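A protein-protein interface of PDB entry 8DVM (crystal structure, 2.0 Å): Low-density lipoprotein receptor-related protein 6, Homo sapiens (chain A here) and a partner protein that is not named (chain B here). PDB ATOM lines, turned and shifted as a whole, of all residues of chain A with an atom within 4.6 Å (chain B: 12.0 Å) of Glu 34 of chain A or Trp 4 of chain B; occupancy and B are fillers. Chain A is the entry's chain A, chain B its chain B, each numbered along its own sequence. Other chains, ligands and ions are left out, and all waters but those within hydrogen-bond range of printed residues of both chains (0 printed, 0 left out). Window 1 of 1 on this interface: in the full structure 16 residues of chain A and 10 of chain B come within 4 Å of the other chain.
Printed residues of chain A that touch a printed residue of chain B: Arg 10, Glu 34, Ile 52, Ser 53, Glu 79, Arg 122, Trp 138 and Trp 221. Hydrophobic or aromatic side chains of chain A within 4 Å of the printed part of chain B: Trp 138 and Trp 221. Of the 15 printed residues of chain B, 8 touch a printed residue of chain A. Hydrophobic or aromatic side chains of chain B that line the printed part of chain A: Trp 4, Phe 5, Trp 8, Phe 9 and Trp 28. Among the printed residues, 15 pairs touch across the chains. Among the printed residues, no Asp or Glu carboxylate lies within 4 Å of a Lys or Arg side-chain nitrogen of the other chain.
The backbone NH (N) of Ala 35 of chain A sits at hydrogen-bond distance from the backbone carbonyl oxygen (O) of Arg 10 of chain A (2.9 Å). The backbone NH (N) of Glu 34 of chain A lies within hydrogen-bond range of the side-chain carboxylate (OD1) of Asp 51 of chain A. The backbone NH (N) of Ile 52 of chain A sits at hydrogen-bond distance from the backbone carbonyl oxygen (O) of Glu 34 of chain A. The side-chain hydroxyl (OG) of Ser 53 of chain A lies within hydrogen-bond range of the side-chain carboxylate (OE1) of Glu 34 of chain A (2.6 Å). The side-chain carboxylate of Asp 51 of chain A lies within hydrogen-bond range of the backbone NH of Ser 53 of chain A, at 3.0 Å. The side-chain sulfur of Cys 2 of chain B is disulfide-bonded to the side-chain sulfur of Cys 29 of chain B, 2.0 Å away.
The side-chain carboxylate (OE1) of Glu 34 of chain A sits at hydrogen-bond distance from the backbone NH (N) of Cys 2 of chain B (3.1 Å). OE1 of Glu 34 of chain A lies within hydrogen-bond range of N of Arg 3 of chain B, at 2.9 Å. OE2 of Glu 34 of chain A sits at hydrogen-bond distance from N of Trp 4 of chain B (3.1 Å). The backbone carbonyl oxygen (O) of Ile 52 of chain A is in hydrogen-bond range of the guanidinium group (NH1) of Arg 3 of chain B, 3.0 Å away. OE1 of Glu 79 of chain A lies within hydrogen-bond range of NE1 of Trp 4 of chain B (2.8 Å). The indole nitrogen (NE1) of Trp 8 of chain B is in hydrogen-bond range of the side-chain carboxylate (OE2) of Glu 79 of chain A (2.9 Å). The guanidinium group of Arg 122 of chain A sits close to the indole nitrogen of Trp 4 of chain B.
Ala 11 of chain A touches none of the printed residues of chain B. No residue of chain B comes within 4 Å of Lys 33 of chain A. No residue of chain B comes within 4 Å of Ala 35 of chain A. Ser 36 of chain A touches none of the printed residues of chain B. No residue of chain B comes within 4 Å of Thr 50 of chain A. Ile 52 of chain A touches just one residue of chain B: Arg 3. Of chain B, only Trp 4 (2.8 Å) and Trp 8 (2.9 Å) come within 4 Å of Glu 79 of chain A. Printed residues of chain B within 4 Å of Trp 221 of chain A: Trp 4, Phe 5 and Phe 9. Of the printed residues of chain A, Trp 4 of chain B touches Glu 34 (3.1 Å), Glu 79 (2.8 Å), Arg 122 (3.4 Å), Trp 138 (3.9 Å) and Trp 221 (3.5 Å). Of the printed residues of chain A, Phe 9 of chain B touches Trp 221. Gly 30 of chain B touches none of the printed residues of chain A. The nearest residue of chain B that does not touch Glu 34 of chain A is Phe 5 of chain B (4.8 Å). The nearest printed residue of chain A that does not touch Trp 4 of chain B is Phe 207 of chain A (4.004 Å).
Among the printed residues, merely in contact across the chains: Arg 10 of chain A with Trp 28 of chain B (3.4 Å), Glu 34 of chain A with Gly 1 of chain B (3.4 Å), Ser 53 of chain A with Gly 1 of chain B (3.2 Å), Trp 138 of chain A with Trp 4 of chain B (3.9 Å), Trp 138 of chain A with Trp 8 of chain B (3.8 Å), Trp 221 of chain A with Trp 4 of chain B (3.5 Å), Trp 221 of chain A with Phe 5 of chain B (3.97 Å) and Trp 221 of chain A with Phe 9 of chain B (3.8 Å).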
ATOM      1  N   ARG A  10      11.317  26.754  17.489  1.00  0.00           N
ATOM      2  CA  ARG A  10      10.164  27.441  18.051  1.00  0.00           C
ATOM      3  C   ARG A  10       8.862  26.858  17.514  1.00  0.00           C
ATOM      4  O   ARG A  10       8.627  25.678  17.644  1.00  0.00           O
ATOM      5  CB  ARG A  10      10.254  28.956  17.869  1.00  0.00           C
ATOM      6  CG  ARG A  10      11.527  29.579  18.404  1.00  0.00           C
ATOM      7  CD  ARG A  10      11.402  31.088  18.487  1.00  0.00           C
ATOM      8  NE  ARG A  10      10.328  31.490  19.389  1.00  0.00           N
ATOM      9  CZ  ARG A  10       9.900  32.739  19.534  1.00  0.00           C
ATOM     10  NH1 ARG A  10      10.459  33.718  18.839  1.00  0.00           N
ATOM     11  NH2 ARG A  10       8.917  33.012  20.379  1.00  0.00           N
ATOM     12  N   ALA A  11       8.027  27.683  16.910  1.00  0.00           N
ATOM     13  CA  ALA A  11       6.781  27.172  16.356  1.00  0.00           C
ATOM     14  C   ALA A  11       6.803  27.099  14.838  1.00  0.00           C
ATOM     15  O   ALA A  11       5.738  27.012  14.218  1.00  0.00           O
ATOM     16  CB  ALA A  11       5.599  28.031  16.821  1.00  0.00           C
ATOM     17  N   VAL A  32       0.898  25.623  15.099  1.00  0.00           N
ATOM     18  CA  VAL A  32       2.053  24.970  15.708  1.00  0.00           C
ATOM     19  C   VAL A  32       2.496  25.779  16.919  1.00  0.00           C
ATOM     20  O   VAL A  32       2.464  27.013  16.899  1.00  0.00           O
ATOM     21  CB  VAL A  32       3.189  24.825  14.679  1.00  0.00           C
ATOM     22  CG1 VAL A  32       4.350  24.029  15.266  1.00  0.00           C
ATOM     23  CG2 VAL A  32       2.686  24.114  13.412  1.00  0.00           C
ATOM     24  N   LYS A  33       2.882  25.097  17.999  1.00  0.00           N
ATOM     25  CA  LYS A  33       3.365  25.832  19.162  1.00  0.00           C
ATOM     26  C   LYS A  33       4.818  25.536  19.495  1.00  0.00           C
ATOM     27  O   LYS A  33       5.572  26.470  19.791  1.00  0.00           O
ATOM     28  CB  LYS A  33       2.481  25.567  20.388  1.00  0.00           C
ATOM     29  CG  LYS A  33       1.271  26.466  20.405  1.00  0.00           C
ATOM     30  CD  LYS A  33       0.289  26.125  21.508  1.00  0.00           C
ATOM     31  CE  LYS A  33       0.901  26.240  22.910  1.00  0.00           C
ATOM     32  NZ  LYS A  33       0.021  25.682  24.005  1.00  0.00           N
ATOM     33  N   GLU A  34       5.228  24.260  19.490  1.00  0.00           N
ATOM     34  CA  GLU A  34       6.603  23.847  19.779  1.00  0.00           C
ATOM     35  C   GLU A  34       6.996  22.690  18.862  1.00  0.00           C
ATOM     36  O   GLU A  34       6.915  21.530  19.261  1.00  0.00           O
ATOM     37  CB  GLU A  34       6.740  23.473  21.247  1.00  0.00           C
ATOM     38  CG  GLU A  34       8.150  23.533  21.798  1.00  0.00           C
ATOM     39  CD  GLU A  34       8.190  23.139  23.262  1.00  0.00           C
ATOM     40  OE1 GLU A  34       7.138  23.275  23.939  1.00  0.00           O
ATOM     41  OE2 GLU A  34       9.233  22.634  23.719  1.00  0.00           O
ATOM     42  N   ALA A  35       7.495  23.023  17.670  1.00  0.00           N
ATOM     43  CA  ALA A  35       7.819  22.007  16.684  1.00  0.00           C
ATOM     44  C   ALA A  35       9.017  21.207  17.155  1.00  0.00           C
ATOM     45  O   ALA A  35       9.990  21.780  17.645  1.00  0.00           O
ATOM     46  CB  ALA A  35       8.090  22.657  15.332  1.00  0.00           C
ATOM     47  N   SER A  36       8.913  19.874  17.117  1.00  0.00           N
ATOM     48  CA  SER A  36      10.061  19.107  17.576  1.00  0.00           C
ATOM     49  C   SER A  36      10.647  18.131  16.551  1.00  0.00           C
ATOM     50  O   SER A  36      11.407  18.561  15.676  1.00  0.00           O
ATOM     51  CB  SER A  36       9.612  18.344  18.826  1.00  0.00           C
ATOM     52  OG  SER A  36      10.666  17.650  19.464  1.00  0.00           O
ATOM     53  N   THR A  50       6.248  16.321  15.428  1.00  0.00           N
ATOM     54  CA  THR A  50       5.671  16.321  16.761  1.00  0.00           C
ATOM     55  C   THR A  50       5.738  17.716  17.373  1.00  0.00           C
ATOM     56  O   THR A  50       6.483  18.597  16.929  1.00  0.00           O
ATOM     57  CB  THR A  50       6.395  15.321  17.668  1.00  0.00           C
ATOM     58  OG1 THR A  50       7.674  15.844  18.018  1.00  0.00           O
ATOM     59  CG2 THR A  50       6.611  14.041  16.908  1.00  0.00           C
ATOM     60  N   ASP A  51       4.949  17.894  18.424  1.00  0.00           N
ATOM     61  CA  ASP A  51       4.817  19.170  19.108  1.00  0.00           C
ATOM     62  C   ASP A  51       4.796  18.867  20.596  1.00  0.00           C
ATOM     63  O   ASP A  51       3.889  18.180  21.075  1.00  0.00           O
ATOM     64  CB  ASP A  51       3.534  19.893  18.672  1.00  0.00           C
ATOM     65  CG  ASP A  51       3.489  21.353  19.110  1.00  0.00           C
ATOM     66  OD1 ASP A  51       3.744  21.642  20.311  1.00  0.00           O
ATOM     67  OD2 ASP A  51       3.145  22.206  18.257  1.00  0.00           O
ATOM     68  N   ILE A  52       5.811  19.341  21.320  1.00  0.00           N
ATOM     69  CA  ILE A  52       5.918  19.031  22.743  1.00  0.00           C
ATOM     70  C   ILE A  52       4.980  19.856  23.600  1.00  0.00           C
ATOM     71  O   ILE A  52       4.650  19.440  24.719  1.00  0.00           O
ATOM     72  CB  ILE A  52       7.369  19.208  23.193  1.00  0.00           C
ATOM     73  CG1 ILE A  52       8.260  18.495  22.184  1.00  0.00           C
ATOM     74  CG2 ILE A  52       7.556  18.724  24.623  1.00  0.00           C
ATOM     75  CD1 ILE A  52       8.198  16.997  22.326  1.00  0.00           C
ATOM     76  N   SER A  53       4.528  21.010  23.109  1.00  0.00           N
ATOM     77  CA  SER A  53       3.579  21.809  23.878  1.00  0.00           C
ATOM     78  C   SER A  53       2.156  21.306  23.716  1.00  0.00           C
ATOM     79  O   SER A  53       1.390  21.293  24.679  1.00  0.00           O
ATOM     80  CB  SER A  53       3.645  23.278  23.455  1.00  0.00           C
ATOM     81  OG  SER A  53       4.639  23.942  24.198  1.00  0.00           O
ATOM     82  N   GLU A  79       9.201  13.053  21.765  1.00  0.00           N
ATOM     83  CA  GLU A  79      10.460  13.618  21.286  1.00  0.00           C
ATOM     84  C   GLU A  79      11.077  12.868  20.103  1.00  0.00           C
ATOM     85  O   GLU A  79      12.055  13.363  19.523  1.00  0.00           O
ATOM     86  CB  GLU A  79      11.459  13.688  22.450  1.00  0.00           C
ATOM     87  CG  GLU A  79      10.942  14.575  23.593  1.00  0.00           C
ATOM     88  CD  GLU A  79      11.898  14.726  24.766  1.00  0.00           C
ATOM     89  OE1 GLU A  79      13.115  14.928  24.537  1.00  0.00           O
ATOM     90  OE2 GLU A  79      11.419  14.679  25.924  1.00  0.00           O
ATOM     91  N   ARG A 122      14.117   8.351  23.320  1.00  0.00           N
ATOM     92  CA  ARG A 122      14.135   9.694  22.749  1.00  0.00           C
ATOM     93  C   ARG A 122      14.204   9.702  21.227  1.00  0.00           C
ATOM     94  O   ARG A 122      13.190   9.952  20.585  1.00  0.00           O
ATOM     95  CB  ARG A 122      15.306  10.484  23.335  1.00  0.00           C
ATOM     96  CG  ARG A 122      15.006  11.949  23.469  1.00  0.00           C
ATOM     97  CD  ARG A 122      15.449  12.740  22.238  1.00  0.00           C
ATOM     98  NE  ARG A 122      14.925  14.097  22.332  1.00  0.00           N
ATOM     99  CZ  ARG A 122      14.975  15.015  21.372  1.00  0.00           C
ATOM    100  NH1 ARG A 122      15.572  14.781  20.216  1.00  0.00           N
ATOM    101  NH2 ARG A 122      14.406  16.201  21.582  1.00  0.00           N
ATOM    102  N   TRP A 138      17.305   8.209  27.365  1.00  0.00           N
ATOM    103  CA  TRP A 138      17.895   9.270  28.177  1.00  0.00           C
ATOM    104  C   TRP A 138      17.651   9.061  29.659  1.00  0.00           C
ATOM    105  O   TRP A 138      17.692  10.027  30.424  1.00  0.00           O
ATOM    106  CB  TRP A 138      17.327  10.639  27.807  1.00  0.00           C
ATOM    107  CG  TRP A 138      17.848  11.202  26.551  1.00  0.00           C
ATOM    108  CD1 TRP A 138      18.620  10.561  25.629  1.00  0.00           C
ATOM    109  CD2 TRP A 138      17.598  12.507  26.032  1.00  0.00           C
ATOM    110  NE1 TRP A 138      18.874  11.386  24.572  1.00  0.00           N
ATOM    111  CE2 TRP A 138      18.262  12.593  24.796  1.00  0.00           C
ATOM    112  CE3 TRP A 138      16.892  13.619  26.500  1.00  0.00           C
ATOM    113  CZ2 TRP A 138      18.231  13.742  24.010  1.00  0.00           C
ATOM    114  CZ3 TRP A 138      16.859  14.760  25.722  1.00  0.00           C
ATOM    115  CH2 TRP A 138      17.526  14.816  24.488  1.00  0.00           C
ATOM    116  N   PHE A 207      23.578  19.183  18.693  1.00  0.00           N
ATOM    117  CA  PHE A 207      22.308  18.673  19.178  1.00  0.00           C
ATOM    118  C   PHE A 207      21.616  17.779  18.163  1.00  0.00           C
ATOM    119  O   PHE A 207      21.408  16.606  18.453  1.00  0.00           O
ATOM    120  CB  PHE A 207      21.368  19.817  19.569  1.00  0.00           C
ATOM    121  CG  PHE A 207      20.103  19.335  20.214  1.00  0.00           C
ATOM    122  CD1 PHE A 207      20.104  18.894  21.522  1.00  0.00           C
ATOM    123  CD2 PHE A 207      18.935  19.253  19.483  1.00  0.00           C
ATOM    124  CE1 PHE A 207      18.934  18.418  22.119  1.00  0.00           C
ATOM    125  CE2 PHE A 207      17.770  18.789  20.064  1.00  0.00           C
ATOM    126  CZ  PHE A 207      17.767  18.368  21.382  1.00  0.00           C
ATOM    127  N   TRP A 221      23.834  24.444  19.363  1.00  0.00           N
ATOM    128  CA  TRP A 221      23.075  25.459  20.092  1.00  0.00           C
ATOM    129  C   TRP A 221      23.941  26.590  20.605  1.00  0.00           C
ATOM    130  O   TRP A 221      23.412  27.668  20.911  1.00  0.00           O
ATOM    131  CB  TRP A 221      22.332  24.844  21.277  1.00  0.00           C
ATOM    132  CG  TRP A 221      21.142  24.030  20.863  1.00  0.00           C
ATOM    133  CD1 TRP A 221      20.747  23.756  19.588  1.00  0.00           C
ATOM    134  CD2 TRP A 221      20.206  23.382  21.729  1.00  0.00           C
ATOM    135  NE1 TRP A 221      19.618  22.978  19.606  1.00  0.00           N
ATOM    136  CE2 TRP A 221      19.266  22.733  20.909  1.00  0.00           C
ATOM    137  CE3 TRP A 221      20.075  23.278  23.116  1.00  0.00           C
ATOM    138  CZ2 TRP A 221      18.187  21.995  21.434  1.00  0.00           C
ATOM    139  CZ3 TRP A 221      19.008  22.543  23.640  1.00  0.00           C
ATOM    140  CH2 TRP A 221      18.081  21.911  22.799  1.00  0.00           C
ATOM    141  N   MET A 248      15.682  22.451  17.048  1.00  0.00           N
ATOM    142  CA  MET A 248      15.324  21.196  17.713  1.00  0.00           C
ATOM    143  C   MET A 248      15.527  19.956  16.856  1.00  0.00           C
ATOM    144  O   MET A 248      15.707  18.867  17.413  1.00  0.00           O
ATOM    145  CB  MET A 248      13.873  21.222  18.184  1.00  0.00           C
ATOM    146  CG  MET A 248      13.471  22.381  19.035  1.00  0.00           C
ATOM    147  SD  MET A 248      14.715  22.694  20.339  1.00  0.00           S
ATOM    148  CE  MET A 248      14.510  21.196  21.294  1.00  0.00           C
ATOM    149  N   GLY B   1       5.110  27.439  24.047  1.00  0.00           N
ATOM    150  CA  GLY B   1       6.320  26.678  23.789  1.00  0.00           C
ATOM    151  C   GLY B   1       7.176  26.473  25.027  1.00  0.00           C
ATOM    152  O   GLY B   1       6.723  26.705  26.148  1.00  0.00           O
ATOM    153  N   CYS B   2       8.396  25.998  24.850  1.00  0.00           N
ATOM    154  CA  CYS B   2       9.327  25.797  25.965  1.00  0.00           C
ATOM    155  C   CYS B   2       9.068  24.672  26.955  1.00  0.00           C
ATOM    156  O   CYS B   2       9.721  24.607  27.983  1.00  0.00           O
ATOM    157  CB  CYS B   2       9.626  27.112  26.674  1.00  0.00           C
ATOM    158  SG  CYS B   2       9.965  28.461  25.531  1.00  0.00           S
ATOM    159  N   ARG B   3       8.164  23.762  26.641  1.00  0.00           N
ATOM    160  CA  ARG B   3       7.960  22.615  27.513  1.00  0.00           C
ATOM    161  C   ARG B   3       9.165  21.697  27.607  1.00  0.00           C
ATOM    162  O   ARG B   3       9.474  21.190  28.668  1.00  0.00           O
ATOM    163  CB  ARG B   3       6.697  21.841  27.158  1.00  0.00           C
ATOM    164  CG  ARG B   3       5.733  21.685  28.303  1.00  0.00           C
ATOM    165  CD  ARG B   3       4.518  20.890  27.887  1.00  0.00           C
ATOM    166  NE  ARG B   3       4.228  19.858  28.865  1.00  0.00           N
ATOM    167  CZ  ARG B   3       4.257  18.560  28.607  1.00  0.00           C
ATOM    168  NH1 ARG B   3       4.561  18.135  27.395  1.00  0.00           N
ATOM    169  NH2 ARG B   3       3.982  17.695  29.564  1.00  0.00           N
ATOM    170  N   TRP B   4       9.838  21.482  26.494  1.00  0.00           N
ATOM    171  CA  TRP B   4      11.011  20.629  26.494  1.00  0.00           C
ATOM    172  C   TRP B   4      12.105  21.189  27.389  1.00  0.00           C
ATOM    173  O   TRP B   4      12.724  20.450  28.137  1.00  0.00           O
ATOM    174  CB  TRP B   4      11.537  20.415  25.074  1.00  0.00           C
ATOM    175  CG  TRP B   4      12.679  19.465  24.966  1.00  0.00           C
ATOM    176  CD1 TRP B   4      12.608  18.147  24.668  1.00  0.00           C
ATOM    177  CD2 TRP B   4      14.069  19.762  25.138  1.00  0.00           C
ATOM    178  NE1 TRP B   4      13.860  17.597  24.655  1.00  0.00           N
ATOM    179  CE2 TRP B   4      14.776  18.570  24.944  1.00  0.00           C
ATOM    180  CE3 TRP B   4      14.782  20.922  25.446  1.00  0.00           C
ATOM    181  CZ2 TRP B   4      16.154  18.500  25.044  1.00  0.00           C
ATOM    182  CZ3 TRP B   4      16.146  20.848  25.554  1.00  0.00           C
ATOM    183  CH2 TRP B   4      16.820  19.648  25.353  1.00  0.00           C
ATOM    184  N   PHE B   5      12.335  22.487  27.323  1.00  0.00           N
ATOM    185  CA  PHE B   5      13.331  23.119  28.185  1.00  0.00           C
ATOM    186  C   PHE B   5      12.948  22.991  29.645  1.00  0.00           C
ATOM    187  O   PHE B   5      13.772  22.730  30.478  1.00  0.00           O
ATOM    188  CB  PHE B   5      13.484  24.591  27.836  1.00  0.00           C
ATOM    189  CG  PHE B   5      14.057  24.839  26.474  1.00  0.00           C
ATOM    190  CD1 PHE B   5      15.299  24.342  26.130  1.00  0.00           C
ATOM    191  CD2 PHE B   5      13.357  25.579  25.542  1.00  0.00           C
ATOM    192  CE1 PHE B   5      15.828  24.569  24.879  1.00  0.00           C
ATOM    193  CE2 PHE B   5      13.880  25.811  24.287  1.00  0.00           C
ATOM    194  CZ  PHE B   5      15.118  25.303  23.955  1.00  0.00           C
ATOM    195  N   MET B   6      11.678  23.156  29.947  1.00  0.00           N
ATOM    196  CA  MET B   6      11.219  23.024  31.323  1.00  0.00           C
ATOM    197  C   MET B   6      11.485  21.649  31.904  1.00  0.00           C
ATOM    198  O   MET B   6      11.786  21.534  33.080  1.00  0.00           O
ATOM    199  CB  MET B   6       9.759  23.403  31.460  1.00  0.00           C
ATOM    200  CG  MET B   6       9.512  24.892  31.582  1.00  0.00           C
ATOM    201  SD  MET B   6       7.750  25.253  31.599  1.00  0.00           S
ATOM    202  CE  MET B   6       7.081  23.609  31.860  1.00  0.00           C
ATOM    203  N   LYS B   7      11.323  20.597  31.122  1.00  0.00           N
ATOM    204  CA  LYS B   7      11.714  19.282  31.602  1.00  0.00           C
ATOM    205  C   LYS B   7      13.199  19.003  31.656  1.00  0.00           C
ATOM    206  O   LYS B   7      13.696  18.462  32.626  1.00  0.00           O
ATOM    207  CB  LYS B   7      11.055  18.192  30.772  1.00  0.00           C
ATOM    208  CG  LYS B   7      11.439  16.782  31.177  1.00  0.00           C
ATOM    209  CD  LYS B   7      10.750  15.744  30.320  1.00  0.00           C
ATOM    210  CE  LYS B   7      11.037  14.352  30.830  1.00  0.00           C
ATOM    211  NZ  LYS B   7      10.130  13.333  30.250  1.00  0.00           N
ATOM    212  N   TRP B   8      13.914  19.390  30.615  1.00  0.00           N
ATOM    213  CA  TRP B   8      15.310  19.015  30.532  1.00  0.00           C
ATOM    214  C   TRP B   8      16.352  20.123  30.812  1.00  0.00           C
ATOM    215  O   TRP B   8      17.535  19.850  30.867  1.00  0.00           O
ATOM    216  CB  TRP B   8      15.591  18.374  29.173  1.00  0.00           C
ATOM    217  CG  TRP B   8      14.784  17.181  28.802  1.00  0.00           C
ATOM    218  CD1 TRP B   8      13.728  17.148  27.948  1.00  0.00           C
ATOM    219  CD2 TRP B   8      15.000  15.835  29.222  1.00  0.00           C
ATOM    220  NE1 TRP B   8      13.259  15.874  27.825  1.00  0.00           N
ATOM    221  CE2 TRP B   8      14.022  15.044  28.600  1.00  0.00           C
ATOM    222  CE3 TRP B   8      15.913  15.223  30.079  1.00  0.00           C
ATOM    223  CZ2 TRP B   8      13.932  13.677  28.806  1.00  0.00           C
ATOM    224  CZ3 TRP B   8      15.821  13.867  30.280  1.00  0.00           C
ATOM    225  CH2 TRP B   8      14.839  13.108  29.648  1.00  0.00           C
ATOM    226  N   PHE B   9      15.914  21.356  30.982  1.00  0.00           N
ATOM    227  CA  PHE B   9      16.852  22.451  31.290  1.00  0.00           C
ATOM    228  C   PHE B   9      16.601  23.078  32.661  1.00  0.00           C
ATOM    229  O   PHE B   9      16.807  22.441  33.696  1.00  0.00           O
ATOM    230  CB  PHE B   9      16.798  23.546  30.218  1.00  0.00           C
ATOM    231  CG  PHE B   9      17.872  23.427  29.172  1.00  0.00           C
ATOM    232  CD1 PHE B   9      18.600  22.250  29.031  1.00  0.00           C
ATOM    233  CD2 PHE B   9      18.196  24.513  28.361  1.00  0.00           C
ATOM    234  CE1 PHE B   9      19.610  22.140  28.077  1.00  0.00           C
ATOM    235  CE2 PHE B   9      19.207  24.416  27.406  1.00  0.00           C
ATOM    236  CZ  PHE B   9      19.918  23.226  27.266  1.00  0.00           C
ATOM    237  N   PRO B  25      18.095  30.026  31.179  1.00  0.00           N
ATOM    238  CA  PRO B  25      17.279  29.480  30.085  1.00  0.00           C
ATOM    239  C   PRO B  25      17.191  30.447  28.897  1.00  0.00           C
ATOM    240  O   PRO B  25      17.558  31.618  29.054  1.00  0.00           O
ATOM    241  CB  PRO B  25      15.911  29.262  30.745  1.00  0.00           C
ATOM    242  CG  PRO B  25      15.867  30.262  31.849  1.00  0.00           C
ATOM    243  CD  PRO B  25      17.281  30.424  32.342  1.00  0.00           C
ATOM    244  N   PRO B  26      16.690  29.970  27.707  1.00  0.00           N
ATOM    245  CA  PRO B  26      16.533  30.920  26.594  1.00  0.00           C
ATOM    246  C   PRO B  26      15.442  31.954  26.724  1.00  0.00           C
ATOM    247  O   PRO B  26      14.482  31.756  27.459  1.00  0.00           O
ATOM    248  CB  PRO B  26      16.162  30.022  25.421  1.00  0.00           C
ATOM    249  CG  PRO B  26      15.583  28.803  26.027  1.00  0.00           C
ATOM    250  CD  PRO B  26      16.435  28.588  27.229  1.00  0.00           C
ATOM    251  N   HIS B  27      15.577  33.050  25.989  1.00  0.00           N
ATOM    252  CA  HIS B  27      14.569  34.103  26.006  1.00  0.00           C
ATOM    253  C   HIS B  27      13.427  33.644  25.147  1.00  0.00           C
ATOM    254  O   HIS B  27      13.536  32.578  24.568  1.00  0.00           O
ATOM    255  CB  HIS B  27      15.127  35.441  25.536  1.00  0.00           C
ATOM    256  CG  HIS B  27      15.337  35.532  24.057  1.00  0.00           C
ATOM    257  ND1 HIS B  27      16.364  34.880  23.408  1.00  0.00           N
ATOM    258  CD2 HIS B  27      14.664  36.217  23.102  1.00  0.00           C
ATOM    259  CE1 HIS B  27      16.308  35.152  22.118  1.00  0.00           C
ATOM    260  NE2 HIS B  27      15.286  35.961  21.905  1.00  0.00           N
ATOM    261  N   TRP B  28      12.300  34.338  25.178  1.00  0.00           N
ATOM    262  CA  TRP B  28      11.090  33.937  24.440  1.00  0.00           C
ATOM    263  C   TRP B  28      10.517  32.694  25.069  1.00  0.00           C
ATOM    264  O   TRP B  28       9.613  32.074  24.516  1.00  0.00           O
ATOM    265  CB  TRP B  28      11.168  33.895  22.884  1.00  0.00           C
ATOM    266  CG  TRP B  28      12.251  33.068  22.175  1.00  0.00           C
ATOM    267  CD1 TRP B  28      13.291  33.557  21.447  1.00  0.00           C
ATOM    268  CD2 TRP B  28      12.371  31.632  22.118  1.00  0.00           C
ATOM    269  NE1 TRP B  28      14.066  32.533  20.962  1.00  0.00           N
ATOM    270  CE2 TRP B  28      13.525  31.341  21.362  1.00  0.00           C
ATOM    271  CE3 TRP B  28      11.635  30.572  22.651  1.00  0.00           C
ATOM    272  CZ2 TRP B  28      13.946  30.040  21.115  1.00  0.00           C
ATOM    273  CZ3 TRP B  28      12.057  29.284  22.407  1.00  0.00           C
ATOM    274  CH2 TRP B  28      13.201  29.028  21.648  1.00  0.00           C
ATOM    275  N   CYS B  29      11.023  32.343  26.241  1.00  0.00           N
ATOM    276  CA  CYS B  29      10.497  31.211  26.960  1.00  0.00           C
ATOM    277  C   CYS B  29       9.982  31.788  28.257  1.00  0.00           C
ATOM    278  O   CYS B  29      10.757  32.335  29.034  1.00  0.00           O
ATOM    279  CB  CYS B  29      11.621  30.233  27.257  1.00  0.00           C
ATOM    280  SG  CYS B  29      11.856  28.982  25.996  1.00  0.00           S
ATOM    281  N   GLY B  30       8.691  31.647  28.520  1.00  0.00           N
ATOM    282  CA  GLY B  30       8.109  32.223  29.721  1.00  0.00           C
ATOM    283  C   GLY B  30       8.159  33.740  29.722  1.00  0.00           C
ATOM    284  O   GLY B  30       8.964  34.362  30.420  1.00  0.00           O
